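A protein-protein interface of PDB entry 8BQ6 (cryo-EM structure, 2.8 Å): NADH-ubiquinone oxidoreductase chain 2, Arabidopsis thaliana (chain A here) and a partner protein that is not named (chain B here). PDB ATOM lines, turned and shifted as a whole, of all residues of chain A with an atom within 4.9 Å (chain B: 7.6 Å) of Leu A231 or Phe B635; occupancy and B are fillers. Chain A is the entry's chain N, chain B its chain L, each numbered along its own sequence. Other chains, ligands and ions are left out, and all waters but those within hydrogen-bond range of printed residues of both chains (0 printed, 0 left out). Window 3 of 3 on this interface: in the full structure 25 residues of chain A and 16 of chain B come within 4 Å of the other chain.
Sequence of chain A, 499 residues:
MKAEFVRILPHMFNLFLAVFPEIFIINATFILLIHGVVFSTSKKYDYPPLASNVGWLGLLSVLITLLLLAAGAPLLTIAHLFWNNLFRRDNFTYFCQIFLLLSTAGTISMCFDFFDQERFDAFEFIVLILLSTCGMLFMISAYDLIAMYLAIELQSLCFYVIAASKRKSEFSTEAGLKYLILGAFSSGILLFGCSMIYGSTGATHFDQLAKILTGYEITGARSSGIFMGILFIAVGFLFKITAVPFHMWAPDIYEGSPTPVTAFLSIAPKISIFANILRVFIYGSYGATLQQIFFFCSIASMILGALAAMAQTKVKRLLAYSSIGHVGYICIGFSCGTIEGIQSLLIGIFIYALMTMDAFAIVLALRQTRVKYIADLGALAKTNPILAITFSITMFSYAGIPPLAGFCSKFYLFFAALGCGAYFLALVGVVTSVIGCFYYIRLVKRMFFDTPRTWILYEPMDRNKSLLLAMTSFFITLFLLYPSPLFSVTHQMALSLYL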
ATOM      1  N   PHE A 227       5.833  32.442 -21.651  1.00  0.00           N
ATOM      2  CA  PHE A 227       5.033  31.531 -20.847  1.00  0.00           C
ATOM      3  C   PHE A 227       3.744  31.152 -21.562  1.00  0.00           C
ATOM      4  O   PHE A 227       3.336  29.982 -21.564  1.00  0.00           O
ATOM      5  CB  PHE A 227       4.732  32.180 -19.500  1.00  0.00           C
ATOM      6  CG  PHE A 227       4.001  31.292 -18.560  1.00  0.00           C
ATOM      7  CD1 PHE A 227       2.654  31.469 -18.319  1.00  0.00           C
ATOM      8  CD2 PHE A 227       4.661  30.263 -17.925  1.00  0.00           C
ATOM      9  CE1 PHE A 227       1.991  30.645 -17.447  1.00  0.00           C
ATOM     10  CE2 PHE A 227       3.998  29.435 -17.064  1.00  0.00           C
ATOM     11  CZ  PHE A 227       2.663  29.620 -16.828  1.00  0.00           C
ATOM     12  N   MET A 228       3.101  32.119 -22.204  1.00  0.00           N
ATOM     13  CA  MET A 228       1.852  31.788 -22.871  1.00  0.00           C
ATOM     14  C   MET A 228       2.065  31.138 -24.221  1.00  0.00           C
ATOM     15  O   MET A 228       1.238  30.317 -24.634  1.00  0.00           O
ATOM     16  CB  MET A 228       0.987  33.026 -22.970  1.00  0.00           C
ATOM     17  CG  MET A 228       0.347  33.118 -21.661  1.00  0.00           C
ATOM     18  SD  MET A 228      -1.212  33.895 -21.436  1.00  0.00           S
ATOM     19  CE  MET A 228      -0.703  34.507 -19.857  1.00  0.00           C
ATOM     20  N   GLY A 229       3.201  31.426 -24.840  1.00  0.00           N
ATOM     21  CA  GLY A 229       3.504  30.692 -26.071  1.00  0.00           C
ATOM     22  C   GLY A 229       3.622  29.232 -25.713  1.00  0.00           C
ATOM     23  O   GLY A 229       3.023  28.418 -26.416  1.00  0.00           O
ATOM     24  N   ILE A 230       4.316  28.931 -24.614  1.00  0.00           N
ATOM     25  CA  ILE A 230       4.474  27.559 -24.143  1.00  0.00           C
ATOM     26  C   ILE A 230       3.120  26.942 -23.819  1.00  0.00           C
ATOM     27  O   ILE A 230       2.846  25.796 -24.184  1.00  0.00           O
ATOM     28  CB  ILE A 230       5.416  27.515 -22.929  1.00  0.00           C
ATOM     29  CG1 ILE A 230       6.829  27.899 -23.354  1.00  0.00           C
ATOM     30  CG2 ILE A 230       5.396  26.140 -22.278  1.00  0.00           C
ATOM     31  CD1 ILE A 230       7.375  27.016 -24.440  1.00  0.00           C
ATOM     32  N   LEU A 231       2.259  27.686 -23.119  1.00  0.00           N
ATOM     33  CA  LEU A 231       0.958  27.134 -22.738  1.00  0.00           C
ATOM     34  C   LEU A 231       0.131  26.752 -23.958  1.00  0.00           C
ATOM     35  O   LEU A 231      -0.493  25.683 -23.995  1.00  0.00           O
ATOM     36  CB  LEU A 231       0.176  28.133 -21.898  1.00  0.00           C
ATOM     37  CG  LEU A 231       0.264  28.089 -20.383  1.00  0.00           C
ATOM     38  CD1 LEU A 231       0.044  29.492 -19.880  1.00  0.00           C
ATOM     39  CD2 LEU A 231      -0.777  27.135 -19.825  1.00  0.00           C
ATOM     40  N   PHE A 232       0.089  27.629 -24.959  1.00  0.00           N
ATOM     41  CA  PHE A 232      -0.720  27.354 -26.141  1.00  0.00           C
ATOM     42  C   PHE A 232      -0.138  26.208 -26.963  1.00  0.00           C
ATOM     43  O   PHE A 232      -0.882  25.355 -27.472  1.00  0.00           O
ATOM     44  CB  PHE A 232      -0.854  28.627 -26.972  1.00  0.00           C
ATOM     45  CG  PHE A 232      -1.896  29.570 -26.451  1.00  0.00           C
ATOM     46  CD1 PHE A 232      -1.772  30.135 -25.195  1.00  0.00           C
ATOM     47  CD2 PHE A 232      -2.992  29.900 -27.218  1.00  0.00           C
ATOM     48  CE1 PHE A 232      -2.730  30.997 -24.709  1.00  0.00           C
ATOM     49  CE2 PHE A 232      -3.951  30.766 -26.736  1.00  0.00           C
ATOM     50  CZ  PHE A 232      -3.817  31.314 -25.480  1.00  0.00           C
ATOM     51  N   ILE A 233       1.188  26.159 -27.090  1.00  0.00           N
ATOM     52  CA  ILE A 233       1.808  25.039 -27.789  1.00  0.00           C
ATOM     53  C   ILE A 233       1.518  23.734 -27.053  1.00  0.00           C
ATOM     54  O   ILE A 233       1.241  22.695 -27.671  1.00  0.00           O
ATOM     55  CB  ILE A 233       3.317  25.299 -27.948  1.00  0.00           C
ATOM     56  CG1 ILE A 233       3.546  26.314 -29.065  1.00  0.00           C
ATOM     57  CG2 ILE A 233       4.060  24.018 -28.263  1.00  0.00           C
ATOM     58  CD1 ILE A 233       4.951  26.818 -29.139  1.00  0.00           C
ATOM     59  N   ALA A 234       1.544  23.778 -25.718  1.00  0.00           N
ATOM     60  CA  ALA A 234       1.237  22.601 -24.914  1.00  0.00           C
ATOM     61  C   ALA A 234      -0.205  22.158 -25.109  1.00  0.00           C
ATOM     62  O   ALA A 234      -0.488  20.958 -25.167  1.00  0.00           O
ATOM     63  CB  ALA A 234       1.513  22.893 -23.439  1.00  0.00           C
ATOM     64  N   VAL A 235      -1.130  23.113 -25.206  1.00  0.00           N
ATOM     65  CA  VAL A 235      -2.526  22.772 -25.476  1.00  0.00           C
ATOM     66  C   VAL A 235      -2.655  22.063 -26.821  1.00  0.00           C
ATOM     67  O   VAL A 235      -3.381  21.066 -26.949  1.00  0.00           O
ATOM     68  CB  VAL A 235      -3.407  24.031 -25.409  1.00  0.00           C
ATOM     69  CG1 VAL A 235      -4.717  23.799 -26.131  1.00  0.00           C
ATOM     70  CG2 VAL A 235      -3.674  24.404 -23.962  1.00  0.00           C
ATOM     71  N   LEU A 238      -1.350  18.530 -26.473  1.00  0.00           N
ATOM     72  CA  LEU A 238      -2.257  17.700 -25.690  1.00  0.00           C
ATOM     73  C   LEU A 238      -3.480  17.304 -26.504  1.00  0.00           C
ATOM     74  O   LEU A 238      -3.988  16.186 -26.361  1.00  0.00           O
ATOM     75  CB  LEU A 238      -2.683  18.420 -24.411  1.00  0.00           C
ATOM     76  CG  LEU A 238      -1.651  18.685 -23.310  1.00  0.00           C
ATOM     77  CD1 LEU A 238      -2.154  19.791 -22.395  1.00  0.00           C
ATOM     78  CD2 LEU A 238      -1.308  17.432 -22.521  1.00  0.00           C
ATOM     79  N   PHE A 246      -8.662  17.688 -23.672  1.00  0.00           N
ATOM     80  CA  PHE A 246      -8.632  17.983 -25.105  1.00  0.00           C
ATOM     81  C   PHE A 246      -8.797  16.724 -25.941  1.00  0.00           C
ATOM     82  O   PHE A 246      -8.174  16.569 -26.993  1.00  0.00           O
ATOM     83  CB  PHE A 246      -7.349  18.716 -25.468  1.00  0.00           C
ATOM     84  CG  PHE A 246      -7.031  19.852 -24.548  1.00  0.00           C
ATOM     85  CD1 PHE A 246      -7.632  21.084 -24.728  1.00  0.00           C
ATOM     86  CD2 PHE A 246      -6.146  19.691 -23.501  1.00  0.00           C
ATOM     87  CE1 PHE A 246      -7.354  22.133 -23.882  1.00  0.00           C
ATOM     88  CE2 PHE A 246      -5.862  20.742 -22.656  1.00  0.00           C
ATOM     89  CZ  PHE A 246      -6.468  21.963 -22.847  1.00  0.00           C
ATOM     90  N   ILE A 293       1.483  20.763 -16.168  1.00  0.00           N
ATOM     91  CA  ILE A 293       0.491  20.603 -17.229  1.00  0.00           C
ATOM     92  C   ILE A 293       0.274  19.123 -17.493  1.00  0.00           C
ATOM     93  O   ILE A 293      -0.840  18.591 -17.366  1.00  0.00           O
ATOM     94  CB  ILE A 293       0.950  21.315 -18.514  1.00  0.00           C
ATOM     95  CG1 ILE A 293       1.043  22.823 -18.326  1.00  0.00           C
ATOM     96  CG2 ILE A 293      -0.011  21.023 -19.652  1.00  0.00           C
ATOM     97  CD1 ILE A 293      -0.179  23.416 -17.750  1.00  0.00           C
ATOM     98  N   CYS A 297      -2.967  16.622 -16.628  1.00  0.00           N
ATOM     99  CA  CYS A 297      -3.647  16.007 -17.764  1.00  0.00           C
ATOM    100  C   CYS A 297      -3.521  14.489 -17.749  1.00  0.00           C
ATOM    101  O   CYS A 297      -4.456  13.794 -18.152  1.00  0.00           O
ATOM    102  CB  CYS A 297      -3.112  16.580 -19.074  1.00  0.00           C
ATOM    103  SG  CYS A 297      -3.676  18.266 -19.403  1.00  0.00           S
ATOM    104  N   LEU B 629     -12.036  25.084 -25.162  1.00  0.00           N
ATOM    105  CA  LEU B 629     -11.918  26.471 -24.734  1.00  0.00           C
ATOM    106  C   LEU B 629     -11.856  26.580 -23.218  1.00  0.00           C
ATOM    107  O   LEU B 629     -11.101  27.394 -22.677  1.00  0.00           O
ATOM    108  CB  LEU B 629     -13.094  27.270 -25.285  1.00  0.00           C
ATOM    109  CG  LEU B 629     -13.088  28.772 -25.050  1.00  0.00           C
ATOM    110  CD1 LEU B 629     -11.722  29.350 -25.360  1.00  0.00           C
ATOM    111  CD2 LEU B 629     -14.148  29.399 -25.924  1.00  0.00           C
ATOM    112  N   LEU B 630     -12.656  25.774 -22.520  1.00  0.00           N
ATOM    113  CA  LEU B 630     -12.636  25.773 -21.064  1.00  0.00           C
ATOM    114  C   LEU B 630     -11.305  25.271 -20.533  1.00  0.00           C
ATOM    115  O   LEU B 630     -10.792  25.792 -19.540  1.00  0.00           O
ATOM    116  CB  LEU B 630     -13.777  24.914 -20.529  1.00  0.00           C
ATOM    117  CG  LEU B 630     -15.172  25.522 -20.610  1.00  0.00           C
ATOM    118  CD1 LEU B 630     -16.178  24.513 -20.100  1.00  0.00           C
ATOM    119  CD2 LEU B 630     -15.245  26.814 -19.817  1.00  0.00           C
ATOM    120  N   GLY B 631     -10.736  24.247 -21.171  1.00  0.00           N
ATOM    121  CA  GLY B 631      -9.415  23.791 -20.775  1.00  0.00           C
ATOM    122  C   GLY B 631      -8.354  24.857 -20.970  1.00  0.00           C
ATOM    123  O   GLY B 631      -7.497  25.061 -20.107  1.00  0.00           O
ATOM    124  N   LEU B 632      -8.403  25.556 -22.105  1.00  0.00           N
ATOM    125  CA  LEU B 632      -7.484  26.670 -22.332  1.00  0.00           C
ATOM    126  C   LEU B 632      -7.640  27.746 -21.263  1.00  0.00           C
ATOM    127  O   LEU B 632      -6.648  28.200 -20.672  1.00  0.00           O
ATOM    128  CB  LEU B 632      -7.725  27.256 -23.720  1.00  0.00           C
ATOM    129  CG  LEU B 632      -6.754  28.303 -24.256  1.00  0.00           C
ATOM    130  CD1 LEU B 632      -5.341  27.761 -24.321  1.00  0.00           C
ATOM    131  CD2 LEU B 632      -7.228  28.735 -25.623  1.00  0.00           C
ATOM    132  N   THR B 633      -8.883  28.162 -21.003  1.00  0.00           N
ATOM    133  CA  THR B 633      -9.145  29.191 -20.003  1.00  0.00           C
ATOM    134  C   THR B 633      -8.664  28.754 -18.629  1.00  0.00           C
ATOM    135  O   THR B 633      -8.057  29.540 -17.895  1.00  0.00           O
ATOM    136  CB  THR B 633     -10.639  29.510 -19.966  1.00  0.00           C
ATOM    137  OG1 THR B 633     -11.037  30.059 -21.226  1.00  0.00           O
ATOM    138  CG2 THR B 633     -10.948  30.510 -18.869  1.00  0.00           C
ATOM    139  N   LEU B 634      -8.927  27.498 -18.271  1.00  0.00           N
ATOM    140  CA  LEU B 634      -8.487  26.956 -16.994  1.00  0.00           C
ATOM    141  C   LEU B 634      -6.972  26.974 -16.876  1.00  0.00           C
ATOM    142  O   LEU B 634      -6.430  27.338 -15.827  1.00  0.00           O
ATOM    143  CB  LEU B 634      -9.019  25.534 -16.844  1.00  0.00           C
ATOM    144  CG  LEU B 634      -8.978  24.895 -15.464  1.00  0.00           C
ATOM    145  CD1 LEU B 634     -10.280  24.172 -15.205  1.00  0.00           C
ATOM    146  CD2 LEU B 634      -7.806  23.941 -15.377  1.00  0.00           C
ATOM    147  N   PHE B 635      -6.272  26.560 -17.935  1.00  0.00           N
ATOM    148  CA  PHE B 635      -4.813  26.594 -17.925  1.00  0.00           C
ATOM    149  C   PHE B 635      -4.311  28.006 -17.679  1.00  0.00           C
ATOM    150  O   PHE B 635      -3.485  28.243 -16.792  1.00  0.00           O
ATOM    151  CB  PHE B 635      -4.270  26.089 -19.259  1.00  0.00           C
ATOM    152  CG  PHE B 635      -4.099  24.607 -19.329  1.00  0.00           C
ATOM    153  CD1 PHE B 635      -4.777  23.769 -18.465  1.00  0.00           C
ATOM    154  CD2 PHE B 635      -3.290  24.048 -20.301  1.00  0.00           C
ATOM    155  CE1 PHE B 635      -4.628  22.401 -18.551  1.00  0.00           C
ATOM    156  CE2 PHE B 635      -3.138  22.685 -20.393  1.00  0.00           C
ATOM    157  CZ  PHE B 635      -3.807  21.860 -19.520  1.00  0.00           C
ATOM    158  N   VAL B 636      -4.807  28.958 -18.466  1.00  0.00           N
ATOM    159  CA  VAL B 636      -4.360  30.341 -18.336  1.00  0.00           C
ATOM    160  C   VAL B 636      -4.625  30.851 -16.927  1.00  0.00           C
ATOM    161  O   VAL B 636      -3.739  31.414 -16.272  1.00  0.00           O
ATOM    162  CB  VAL B 636      -5.045  31.217 -19.400  1.00  0.00           C
ATOM    163  CG1 VAL B 636      -4.862  32.688 -19.090  1.00  0.00           C
ATOM    164  CG2 VAL B 636      -4.481  30.890 -20.763  1.00  0.00           C
ATOM    165  N   THR B 637      -5.833  30.606 -16.421  1.00  0.00           N
ATOM    166  CA  THR B 637      -6.212  31.111 -15.109  1.00  0.00           C
ATOM    167  C   THR B 637      -5.334  30.516 -14.017  1.00  0.00           C
ATOM    168  O   THR B 637      -4.732  31.247 -13.223  1.00  0.00           O
ATOM    169  CB  THR B 637      -7.686  30.806 -14.848  1.00  0.00           C
ATOM    170  OG1 THR B 637      -8.496  31.745 -15.564  1.00  0.00           O
ATOM    171  CG2 THR B 637      -8.003  30.907 -13.366  1.00  0.00           C
ATOM    172  N   PHE B 638      -5.224  29.189 -13.975  1.00  0.00           N
ATOM    173  CA  PHE B 638      -4.516  28.572 -12.863  1.00  0.00           C
ATOM    174  C   PHE B 638      -3.013  28.789 -12.963  1.00  0.00           C
ATOM    175  O   PHE B 638      -2.370  29.135 -11.966  1.00  0.00           O
ATOM    176  CB  PHE B 638      -4.830  27.080 -12.785  1.00  0.00           C
ATOM    177  CG  PHE B 638      -4.042  26.362 -11.728  1.00  0.00           C
ATOM    178  CD1 PHE B 638      -2.813  25.792 -12.017  1.00  0.00           C
ATOM    179  CD2 PHE B 638      -4.520  26.281 -10.435  1.00  0.00           C
ATOM    180  CE1 PHE B 638      -2.086  25.148 -11.040  1.00  0.00           C
ATOM    181  CE2 PHE B 638      -3.797  25.635  -9.458  1.00  0.00           C
ATOM    182  CZ  PHE B 638      -2.580  25.068  -9.761  1.00  0.00           C
ATOM    183  N   PHE B 639      -2.423  28.580 -14.138  1.00  0.00           N
ATOM    184  CA  PHE B 639      -0.974  28.594 -14.223  1.00  0.00           C
ATOM    185  C   PHE B 639      -0.394  29.966 -14.537  1.00  0.00           C
ATOM    186  O   PHE B 639       0.831  30.116 -14.496  1.00  0.00           O
ATOM    187  CB  PHE B 639      -0.457  27.580 -15.262  1.00  0.00           C
ATOM    188  CG  PHE B 639      -0.974  26.176 -15.068  1.00  0.00           C
ATOM    189  CD1 PHE B 639      -0.106  25.164 -14.703  1.00  0.00           C
ATOM    190  CD2 PHE B 639      -2.286  25.843 -15.358  1.00  0.00           C
ATOM    191  CE1 PHE B 639      -0.560  23.874 -14.527  1.00  0.00           C
ATOM    192  CE2 PHE B 639      -2.740  24.547 -15.206  1.00  0.00           C
ATOM    193  CZ  PHE B 639      -1.876  23.563 -14.794  1.00  0.00           C
ATOM    194  N   CYS B 640      -1.214  30.965 -14.852  1.00  0.00           N
ATOM    195  CA  CYS B 640      -0.631  32.302 -14.911  1.00  0.00           C
ATOM    196  C   CYS B 640      -1.281  33.280 -13.945  1.00  0.00           C
ATOM    197  O   CYS B 640      -0.571  33.934 -13.179  1.00  0.00           O
ATOM    198  CB  CYS B 640      -0.702  32.864 -16.336  1.00  0.00           C
ATOM    199  SG  CYS B 640       0.620  34.044 -16.703  1.00  0.00           S
ATOM    200  N   MET B 641      -2.610  33.393 -13.953  1.00  0.00           N
ATOM    201  CA  MET B 641      -3.313  34.245 -12.993  1.00  0.00           C
ATOM    202  C   MET B 641      -3.550  33.500 -11.684  1.00  0.00           C
ATOM    203  O   MET B 641      -4.677  33.179 -11.319  1.00  0.00           O
ATOM    204  CB  MET B 641      -4.642  34.730 -13.557  1.00  0.00           C
ATOM    205  CG  MET B 641      -4.584  35.960 -14.417  1.00  0.00           C
ATOM    206  SD  MET B 641      -5.558  35.698 -15.906  1.00  0.00           S
ATOM    207  CE  MET B 641      -7.192  35.564 -15.204  1.00  0.00           C
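The backbone carbonyl oxygen of Ile A293 lies close to the side-chain sulfur of Cys A297.
Phe A227 touches Phe B639.
Phe A227 touches Cys B640.
Met A228 touches Cys B640 (CE to SG, 3.5 Å).
Val A235 touches Leu B632.
CE2 of Phe B635 touches CD1 of Leu A238, 3.7 Å away.
Gly B631 touches Phe A246 (C to CZ, 3.9 Å).
Phe A246 touches Leu B632.
Phe A246 touches Phe B635 (CE2 to CZ, 3.9 Å).
Ile A293 touches Phe B635.
Cys A297 touches Phe B635 (SG to CZ, 3.6 Å).
Printed residues of chain B within 4 Å of Phe A227: Phe B639 and Cys B640.
Printed residues of chain B within 4 Å of Met A228: Cys B640.
Printed residues of chain B within 4 Å of Leu A231: Phe B635 (3.7 Å).
Printed residues of chain B within 4 Å of Val A235: Leu B632 (3.8 Å) and Phe B635 (3.7 Å).
Of the printed residues of chain B, Phe A246 touches Gly B631 (3.9 Å), Leu B632 (3.997 Å) and Phe B635 (3.9 Å).
Printed residues of chain B within 4 Å of Cys A297: Phe B635.
Thr B633 touches none of the printed residues of chain A.
Of the printed residues of chain A, Phe B635 touches Leu A231 (3.7 Å), Val A235 (3.7 Å), Leu A238 (3.7 Å), Phe A246 (3.9 Å), Ile A293 (3.6 Å) and Cys A297 (3.6 Å).
The nearest residue of chain B that does not touch Leu A231 is Phe B639 (4.6 Å).
Of the 13 printed residues of chain B, 5 touch a printed residue of chain A.
Of the 13 printed residues of chain A, 8 touch a printed residue of chain B.
Hydrophobic or aromatic side chains of chain A that line the printed part of chain B: Phe A227, Met A228, Leu A231, Val A235, Leu A238, Phe A246 and Ile A293.
Among the printed residues, no Asp or Glu carboxylate lies within 4 Å of a Lys or Arg side-chain nitrogen of the other chain.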
